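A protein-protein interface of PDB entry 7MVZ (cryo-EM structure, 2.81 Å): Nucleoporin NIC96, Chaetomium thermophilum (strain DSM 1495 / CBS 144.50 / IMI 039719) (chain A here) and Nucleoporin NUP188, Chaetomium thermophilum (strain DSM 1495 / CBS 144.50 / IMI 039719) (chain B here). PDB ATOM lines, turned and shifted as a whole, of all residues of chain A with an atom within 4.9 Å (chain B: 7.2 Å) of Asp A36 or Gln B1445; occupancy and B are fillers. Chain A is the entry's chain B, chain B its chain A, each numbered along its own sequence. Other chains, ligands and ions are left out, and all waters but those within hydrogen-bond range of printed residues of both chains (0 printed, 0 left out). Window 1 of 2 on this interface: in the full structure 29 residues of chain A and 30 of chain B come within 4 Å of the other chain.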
ATOM      1  N   ARG A  32      -2.234   9.465 -14.219  1.00  0.00           N
ATOM      2  CA  ARG A  32      -1.786  10.289 -15.339  1.00  0.00           C
ATOM      3  C   ARG A  32      -2.826  11.337 -15.718  1.00  0.00           C
ATOM      4  O   ARG A  32      -2.481  12.490 -15.998  1.00  0.00           O
ATOM      5  CB  ARG A  32      -1.448   9.407 -16.542  1.00  0.00           C
ATOM      6  CG  ARG A  32      -0.902  10.183 -17.733  1.00  0.00           C
ATOM      7  CD  ARG A  32      -0.435   9.268 -18.858  1.00  0.00           C
ATOM      8  NE  ARG A  32      -1.520   8.465 -19.415  1.00  0.00           N
ATOM      9  CZ  ARG A  32      -1.851   7.246 -18.996  1.00  0.00           C
ATOM     10  NH1 ARG A  32      -1.185   6.667 -18.005  1.00  0.00           N
ATOM     11  NH2 ARG A  32      -2.856   6.601 -19.572  1.00  0.00           N
ATOM     12  N   SER A  33      -4.104  10.955 -15.754  1.00  0.00           N
ATOM     13  CA  SER A  33      -5.155  11.924 -16.048  1.00  0.00           C
ATOM     14  C   SER A  33      -5.215  13.017 -14.987  1.00  0.00           C
ATOM     15  O   SER A  33      -5.371  14.201 -15.311  1.00  0.00           O
ATOM     16  CB  SER A  33      -6.504  11.215 -16.161  1.00  0.00           C
ATOM     17  OG  SER A  33      -7.533  12.126 -16.504  1.00  0.00           O
ATOM     18  N   ALA A  34      -5.141  12.631 -13.712  1.00  0.00           N
ATOM     19  CA  ALA A  34      -5.155  13.615 -12.633  1.00  0.00           C
ATOM     20  C   ALA A  34      -3.966  14.565 -12.713  1.00  0.00           C
ATOM     21  O   ALA A  34      -4.058  15.714 -12.266  1.00  0.00           O
ATOM     22  CB  ALA A  34      -5.172  12.906 -11.279  1.00  0.00           C
ATOM     23  N   ARG A  35      -2.848  14.110 -13.276  1.00  0.00           N
ATOM     24  CA  ARG A  35      -1.672  14.962 -13.421  1.00  0.00           C
ATOM     25  C   ARG A  35      -1.692  15.782 -14.702  1.00  0.00           C
ATOM     26  O   ARG A  35      -1.000  16.804 -14.782  1.00  0.00           O
ATOM     27  CB  ARG A  35      -0.394  14.116 -13.380  1.00  0.00           C
ATOM     28  CG  ARG A  35      -0.214  13.331 -12.091  1.00  0.00           C
ATOM     29  CD  ARG A  35       1.055  12.496 -12.121  1.00  0.00           C
ATOM     30  NE  ARG A  35       1.230  11.724 -10.894  1.00  0.00           N
ATOM     31  CZ  ARG A  35       2.252  10.904 -10.663  1.00  0.00           C
ATOM     32  NH1 ARG A  35       3.201  10.743 -11.576  1.00  0.00           N
ATOM     33  NH2 ARG A  35       2.324  10.244  -9.515  1.00  0.00           N
ATOM     34  N   ASP A  36      -2.467  15.356 -15.699  1.00  0.00           N
ATOM     35  CA  ASP A  36      -2.587  16.108 -16.943  1.00  0.00           C
ATOM     36  C   ASP A  36      -3.636  17.203 -16.817  1.00  0.00           C
ATOM     37  O   ASP A  36      -3.483  18.286 -17.394  1.00  0.00           O
ATOM     38  CB  ASP A  36      -2.933  15.166 -18.097  1.00  0.00           C
ATOM     39  CG  ASP A  36      -1.867  14.116 -18.333  1.00  0.00           C
ATOM     40  OD1 ASP A  36      -0.859  14.114 -17.596  1.00  0.00           O
ATOM     41  OD2 ASP A  36      -2.035  13.292 -19.257  1.00  0.00           O
ATOM     42  N   PHE A  37      -4.724  16.912 -16.099  1.00  0.00           N
ATOM     43  CA  PHE A  37      -5.791  17.887 -15.894  1.00  0.00           C
ATOM     44  C   PHE A  37      -5.254  19.219 -15.388  1.00  0.00           C
ATOM     45  O   PHE A  37      -5.749  20.279 -15.779  1.00  0.00           O
ATOM     46  CB  PHE A  37      -6.825  17.326 -14.916  1.00  0.00           C
ATOM     47  CG  PHE A  37      -7.986  18.247 -14.669  1.00  0.00           C
ATOM     48  CD1 PHE A  37      -9.097  18.220 -15.496  1.00  0.00           C
ATOM     49  CD2 PHE A  37      -7.969  19.137 -13.608  1.00  0.00           C
ATOM     50  CE1 PHE A  37     -10.167  19.064 -15.271  1.00  0.00           C
ATOM     51  CE2 PHE A  37      -9.036  19.984 -13.379  1.00  0.00           C
ATOM     52  CZ  PHE A  37     -10.136  19.947 -14.212  1.00  0.00           C
ATOM     53  N   ASP A  38      -4.301  19.189 -14.455  1.00  0.00           N
ATOM     54  CA  ASP A  38      -3.712  20.430 -13.956  1.00  0.00           C
ATOM     55  C   ASP A  38      -3.152  21.282 -15.094  1.00  0.00           C
ATOM     56  O   ASP A  38      -3.505  22.459 -15.241  1.00  0.00           O
ATOM     57  CB  ASP A  38      -2.621  20.110 -12.933  1.00  0.00           C
ATOM     58  CG  ASP A  38      -3.152  19.345 -11.735  1.00  0.00           C
ATOM     59  OD1 ASP A  38      -4.335  19.535 -11.384  1.00  0.00           O
ATOM     60  OD2 ASP A  38      -2.385  18.556 -11.145  1.00  0.00           O
ATOM     61  N   ALA A  39      -2.242  20.711 -15.889  1.00  0.00           N
ATOM     62  CA  ALA A  39      -1.690  21.440 -17.028  1.00  0.00           C
ATOM     63  C   ALA A  39      -2.775  21.869 -18.008  1.00  0.00           C
ATOM     64  O   ALA A  39      -2.678  22.944 -18.614  1.00  0.00           O
ATOM     65  CB  ALA A  39      -0.646  20.583 -17.741  1.00  0.00           C
ATOM     66  N   PHE A  40      -3.833  21.070 -18.149  1.00  0.00           N
ATOM     67  CA  PHE A  40      -4.898  21.427 -19.080  1.00  0.00           C
ATOM     68  C   PHE A  40      -5.672  22.638 -18.575  1.00  0.00           C
ATOM     69  O   PHE A  40      -6.021  23.531 -19.354  1.00  0.00           O
ATOM     70  CB  PHE A  40      -5.819  20.224 -19.295  1.00  0.00           C
ATOM     71  CG  PHE A  40      -7.014  20.512 -20.158  1.00  0.00           C
ATOM     72  CD1 PHE A  40      -6.897  20.532 -21.539  1.00  0.00           C
ATOM     73  CD2 PHE A  40      -8.263  20.710 -19.595  1.00  0.00           C
ATOM     74  CE1 PHE A  40      -7.997  20.780 -22.338  1.00  0.00           C
ATOM     75  CE2 PHE A  40      -9.367  20.955 -20.393  1.00  0.00           C
ATOM     76  CZ  PHE A  40      -9.232  20.990 -21.764  1.00  0.00           C
ATOM     77  N   GLY B1438     -15.211  10.966 -11.798  1.00  0.00           N
ATOM     78  CA  GLY B1438     -13.942  11.051 -12.499  1.00  0.00           C
ATOM     79  C   GLY B1438     -13.975  10.420 -13.877  1.00  0.00           C
ATOM     80  O   GLY B1438     -13.226  10.829 -14.767  1.00  0.00           O
ATOM     81  N   LEU B1439     -14.841   9.426 -14.076  1.00  0.00           N
ATOM     82  CA  LEU B1439     -14.989   8.824 -15.398  1.00  0.00           C
ATOM     83  C   LEU B1439     -15.406   9.873 -16.423  1.00  0.00           C
ATOM     84  O   LEU B1439     -14.703  10.113 -17.413  1.00  0.00           O
ATOM     85  CB  LEU B1439     -16.010   7.683 -15.326  1.00  0.00           C
ATOM     86  CG  LEU B1439     -16.091   6.672 -16.475  1.00  0.00           C
ATOM     87  CD1 LEU B1439     -16.935   5.481 -16.051  1.00  0.00           C
ATOM     88  CD2 LEU B1439     -16.653   7.277 -17.749  1.00  0.00           C
ATOM     89  N   ALA B1440     -16.559  10.510 -16.200  1.00  0.00           N
ATOM     90  CA  ALA B1440     -17.001  11.570 -17.097  1.00  0.00           C
ATOM     91  C   ALA B1440     -16.007  12.722 -17.125  1.00  0.00           C
ATOM     92  O   ALA B1440     -15.842  13.376 -18.161  1.00  0.00           O
ATOM     93  CB  ALA B1440     -18.382  12.071 -16.679  1.00  0.00           C
ATOM     94  N   LEU B1441     -15.330  12.979 -16.004  1.00  0.00           N
ATOM     95  CA  LEU B1441     -14.336  14.044 -15.962  1.00  0.00           C
ATOM     96  C   LEU B1441     -13.246  13.802 -16.999  1.00  0.00           C
ATOM     97  O   LEU B1441     -12.978  14.655 -17.851  1.00  0.00           O
ATOM     98  CB  LEU B1441     -13.744  14.137 -14.553  1.00  0.00           C
ATOM     99  CG  LEU B1441     -12.959  15.390 -14.149  1.00  0.00           C
ATOM    100  CD1 LEU B1441     -12.706  15.359 -12.651  1.00  0.00           C
ATOM    101  CD2 LEU B1441     -11.641  15.538 -14.900  1.00  0.00           C
ATOM    102  N   THR B1442     -12.607  12.631 -16.941  1.00  0.00           N
ATOM    103  CA  THR B1442     -11.540  12.325 -17.889  1.00  0.00           C
ATOM    104  C   THR B1442     -12.074  12.186 -19.308  1.00  0.00           C
ATOM    105  O   THR B1442     -11.376  12.540 -20.268  1.00  0.00           O
ATOM    106  CB  THR B1442     -10.797  11.052 -17.471  1.00  0.00           C
ATOM    107  OG1 THR B1442      -9.710  10.813 -18.375  1.00  0.00           O
ATOM    108  CG2 THR B1442     -11.724   9.843 -17.471  1.00  0.00           C
ATOM    109  N   LEU B1443     -13.300  11.679 -19.470  1.00  0.00           N
ATOM    110  CA  LEU B1443     -13.885  11.608 -20.805  1.00  0.00           C
ATOM    111  C   LEU B1443     -13.977  12.994 -21.431  1.00  0.00           C
ATOM    112  O   LEU B1443     -13.504  13.212 -22.552  1.00  0.00           O
ATOM    113  CB  LEU B1443     -15.263  10.948 -20.751  1.00  0.00           C
ATOM    114  CG  LEU B1443     -15.311   9.442 -20.476  1.00  0.00           C
ATOM    115  CD1 LEU B1443     -16.754   8.963 -20.501  1.00  0.00           C
ATOM    116  CD2 LEU B1443     -14.467   8.653 -21.470  1.00  0.00           C
ATOM    117  N   LEU B1444     -14.581  13.947 -20.717  1.00  0.00           N
ATOM    118  CA  LEU B1444     -14.694  15.296 -21.259  1.00  0.00           C
ATOM    119  C   LEU B1444     -13.325  15.942 -21.415  1.00  0.00           C
ATOM    120  O   LEU B1444     -13.106  16.704 -22.362  1.00  0.00           O
ATOM    121  CB  LEU B1444     -15.586  16.151 -20.359  1.00  0.00           C
ATOM    122  CG  LEU B1444     -17.040  15.694 -20.210  1.00  0.00           C
ATOM    123  CD1 LEU B1444     -17.776  16.585 -19.222  1.00  0.00           C
ATOM    124  CD2 LEU B1444     -17.759  15.682 -21.553  1.00  0.00           C
ATOM    125  N   GLN B1445     -12.396  15.650 -20.504  1.00  0.00           N
ATOM    126  CA  GLN B1445     -11.022  16.119 -20.640  1.00  0.00           C
ATOM    127  C   GLN B1445     -10.438  15.737 -21.994  1.00  0.00           C
ATOM    128  O   GLN B1445      -9.991  16.592 -22.767  1.00  0.00           O
ATOM    129  CB  GLN B1445     -10.168  15.544 -19.508  1.00  0.00           C
ATOM    130  CG  GLN B1445      -8.761  16.110 -19.444  1.00  0.00           C
ATOM    131  CD  GLN B1445      -7.999  15.631 -18.226  1.00  0.00           C
ATOM    132  OE1 GLN B1445      -8.550  14.947 -17.364  1.00  0.00           O
ATOM    133  NE2 GLN B1445      -6.718  15.972 -18.160  1.00  0.00           N
ATOM    134  N   ARG B1446     -10.412  14.433 -22.281  1.00  0.00           N
ATOM    135  CA  ARG B1446      -9.838  13.957 -23.535  1.00  0.00           C
ATOM    136  C   ARG B1446     -10.633  14.431 -24.748  1.00  0.00           C
ATOM    137  O   ARG B1446     -10.045  14.724 -25.797  1.00  0.00           O
ATOM    138  CB  ARG B1446      -9.745  12.432 -23.507  1.00  0.00           C
ATOM    139  CG  ARG B1446      -8.864  11.912 -22.380  1.00  0.00           C
ATOM    140  CD  ARG B1446      -8.813  10.399 -22.357  1.00  0.00           C
ATOM    141  NE  ARG B1446      -7.988   9.893 -21.261  1.00  0.00           N
ATOM    142  CZ  ARG B1446      -6.668   9.749 -21.315  1.00  0.00           C
ATOM    143  NH1 ARG B1446      -5.998  10.074 -22.413  1.00  0.00           N
ATOM    144  NH2 ARG B1446      -6.012   9.280 -20.262  1.00  0.00           N
ATOM    145  N   LEU B1447     -11.961  14.524 -24.638  1.00  0.00           N
ATOM    146  CA  LEU B1447     -12.735  15.019 -25.774  1.00  0.00           C
ATOM    147  C   LEU B1447     -12.447  16.490 -26.051  1.00  0.00           C
ATOM    148  O   LEU B1447     -12.493  16.920 -27.208  1.00  0.00           O
ATOM    149  CB  LEU B1447     -14.231  14.803 -25.544  1.00  0.00           C
ATOM    150  CG  LEU B1447     -14.785  13.485 -26.100  1.00  0.00           C
ATOM    151  CD1 LEU B1447     -14.203  12.274 -25.386  1.00  0.00           C
ATOM    152  CD2 LEU B1447     -16.304  13.477 -26.028  1.00  0.00           C
ATOM    153  N   ALA B1448     -12.153  17.271 -25.010  1.00  0.00           N
ATOM    154  CA  ALA B1448     -11.749  18.656 -25.221  1.00  0.00           C
ATOM    155  C   ALA B1448     -10.346  18.726 -25.803  1.00  0.00           C
ATOM    156  O   ALA B1448     -10.065  19.561 -26.670  1.00  0.00           O
ATOM    157  CB  ALA B1448     -11.827  19.431 -23.906  1.00  0.00           C
ATOM    158  N   ASP B1449      -9.449  17.856 -25.334  1.00  0.00           N
ATOM    159  CA  ASP B1449      -8.118  17.778 -25.928  1.00  0.00           C
ATOM    160  C   ASP B1449      -8.206  17.457 -27.414  1.00  0.00           C
ATOM    161  O   ASP B1449      -7.399  17.947 -28.213  1.00  0.00           O
ATOM    162  CB  ASP B1449      -7.281  16.722 -25.205  1.00  0.00           C
ATOM    163  CG  ASP B1449      -7.080  17.041 -23.737  1.00  0.00           C
ATOM    164  OD1 ASP B1449      -7.592  18.082 -23.280  1.00  0.00           O
ATOM    165  OD2 ASP B1449      -6.409  16.249 -23.043  1.00  0.00           O
ATOM    166  N   ALA B1450      -9.183  16.636 -27.804  1.00  0.00           N
ATOM    167  CA  ALA B1450      -9.410  16.344 -29.213  1.00  0.00           C
ATOM    168  C   ALA B1450     -10.258  17.405 -29.902  1.00  0.00           C
ATOM    169  O   ALA B1450     -10.193  17.530 -31.129  1.00  0.00           O
ATOM    170  CB  ALA B1450     -10.079  14.977 -29.365  1.00  0.00           C
ATOM    171  N   ASN B1451     -11.049  18.165 -29.145  1.00  0.00           N
ATOM    172  CA  ASN B1451     -11.878  19.239 -29.691  1.00  0.00           C
ATOM    173  C   ASN B1451     -12.849  18.694 -30.742  1.00  0.00           C
ATOM    174  O   ASN B1451     -12.859  19.114 -31.901  1.00  0.00           O
ATOM    175  CB  ASN B1451     -11.003  20.354 -30.274  1.00  0.00           C
ATOM    176  CG  ASN B1451     -10.064  20.955 -29.249  1.00  0.00           C
ATOM    177  OD1 ASN B1451     -10.406  21.919 -28.564  1.00  0.00           O
ATOM    178  ND2 ASN B1451      -8.869  20.385 -29.135  1.00  0.00           N
ATOM    179  N   VAL B1492     -15.322  21.614 -16.977  1.00  0.00           N
ATOM    180  CA  VAL B1492     -15.123  21.138 -18.345  1.00  0.00           C
ATOM    181  C   VAL B1492     -16.394  21.310 -19.168  1.00  0.00           C
ATOM    182  O   VAL B1492     -16.330  21.605 -20.368  1.00  0.00           O
ATOM    183  CB  VAL B1492     -14.638  19.673 -18.351  1.00  0.00           C
ATOM    184  CG1 VAL B1492     -13.272  19.566 -17.690  1.00  0.00           C
ATOM    185  CG2 VAL B1492     -15.637  18.762 -17.659  1.00  0.00           C
ATOM    186  N   ARG B1495     -16.649  24.898 -20.135  1.00  0.00           N
ATOM    187  CA  ARG B1495     -15.621  25.178 -21.131  1.00  0.00           C
ATOM    188  C   ARG B1495     -16.052  24.691 -22.508  1.00  0.00           C
ATOM    189  O   ARG B1495     -15.892  25.406 -23.504  1.00  0.00           O
ATOM    190  CB  ARG B1495     -14.297  24.529 -20.725  1.00  0.00           C
ATOM    191  CG  ARG B1495     -13.150  24.840 -21.676  1.00  0.00           C
ATOM    192  CD  ARG B1495     -11.872  24.130 -21.271  1.00  0.00           C
ATOM    193  NE  ARG B1495     -10.771  24.437 -22.182  1.00  0.00           N
ATOM    194  CZ  ARG B1495     -10.582  23.847 -23.359  1.00  0.00           C
ATOM    195  NH1 ARG B1495     -11.421  22.911 -23.784  1.00  0.00           N
ATOM    196  NH2 ARG B1495      -9.550  24.196 -24.115  1.00  0.00           N
ATOM    197  N   GLU B1811       3.836  18.564 -19.221  1.00  0.00           N
ATOM    198  CA  GLU B1811       3.062  17.526 -19.886  1.00  0.00           C
ATOM    199  C   GLU B1811       2.825  17.817 -21.362  1.00  0.00           C
ATOM    200  O   GLU B1811       2.190  17.004 -22.043  1.00  0.00           O
ATOM    201  CB  GLU B1811       1.713  17.335 -19.180  1.00  0.00           C
ATOM    202  CG  GLU B1811       1.814  16.773 -17.768  1.00  0.00           C
ATOM    203  CD  GLU B1811       2.366  17.773 -16.771  1.00  0.00           C
ATOM    204  OE1 GLU B1811       2.612  18.933 -17.164  1.00  0.00           O
ATOM    205  OE2 GLU B1811       2.556  17.399 -15.595  1.00  0.00           O
ATOM    206  N   VAL B1812       3.309  18.945 -21.871  1.00  0.00           N
ATOM    207  CA  VAL B1812       3.123  19.299 -23.273  1.00  0.00           C
ATOM    208  C   VAL B1812       4.396  19.932 -23.822  1.00  0.00           C
ATOM    209  O   VAL B1812       5.251  20.387 -23.063  1.00  0.00           O
ATOM    210  CB  VAL B1812       1.921  20.248 -23.456  1.00  0.00           C
ATOM    211  CG1 VAL B1812       0.624  19.545 -23.078  1.00  0.00           C
ATOM    212  CG2 VAL B1812       2.105  21.515 -22.631  1.00  0.00           C
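Among the printed residues, pairs that only touch across the chains: Phe A40 with Asp B1449 (2.9 Å), Phe A40 with Arg B1495 (3.5 Å), Asp A36 with Gln B1445 (3.6 Å), Arg A35 with Glu B1811 (3.7 Å), Ala A39 with Glu B1811 (3.7 Å), Phe A40 with Ala B1448 (3.7 Å), Phe A37 with Leu B1441 (3.7 Å), Asp A36 with Glu B1811 (3.8 Å) and Phe A37 with Val B1492 (3.97 Å).
The side-chain hydroxyl of Ser A33 is in hydrogen-bond range of the side-chain hydroxyl of Thr B1442, at 3.2 Å.
OE1 of Gln B1445 is in hydrogen-bond range of OG of Ser A33, 3.1 Å away.
The side-chain amide nitrogen of Gln B1445 lies close to the backbone NH of Phe A37 (3.0 Å).
Of the printed residues of chain B, Asp A36 touches Gln B1445 and Glu B1811.
Of chain A, only Ser A33, Asp A36 and Phe A37 come within 4 Å of Gln B1445.
Printed residues of chain B within 4 Å of Arg A35: Glu B1811 (3.7 Å).
Of the printed residues of chain B, Phe A40 touches Ala B1448, Asp B1449 and Arg B1495.
Leu B1439 touches none of the printed residues of chain A.
The nearest residue of chain B that does not touch Asp A36 is Arg B1446 (5.7 Å).
The nearest residue of chain A that does not touch Gln B1445 is Phe A40 (4.5 Å).
The nearest printed residue of chain B that does not touch Phe A37 is Glu B1811 (6.7 Å).
The side-chain hydroxyl (OG1) of Thr B1442 sits at hydrogen-bond distance from the guanidinium group (NE) of Arg B1446 (3.5 Å).
O of Ala B1448 sits at hydrogen-bond distance from ND2 of Asn B1451.
The backbone carbonyl oxygen (O) of Asp B1449 sits at hydrogen-bond distance from the side-chain amide nitrogen (ND2) of Asn B1451, 3.0 Å away.
Of the 9 printed residues of chain A, 6 touch a printed residue of chain B.
Of the 18 printed residues of chain B, 8 touch a printed residue of chain A.
Hydrophobic or aromatic side chains of chain B within 4 Å of the printed part of chain A: Leu B1441, Ala B1448 and Val B1492.
Along chain B the printed residues that touch a printed residue of chain A span positions 1441 to 1811.
Among the printed residues, 12 pairs touch across the chains.
Among the printed residues, no Asp or Glu carboxylate lies within 4 Å of a Lys or Arg side-chain nitrogen of the other chain.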
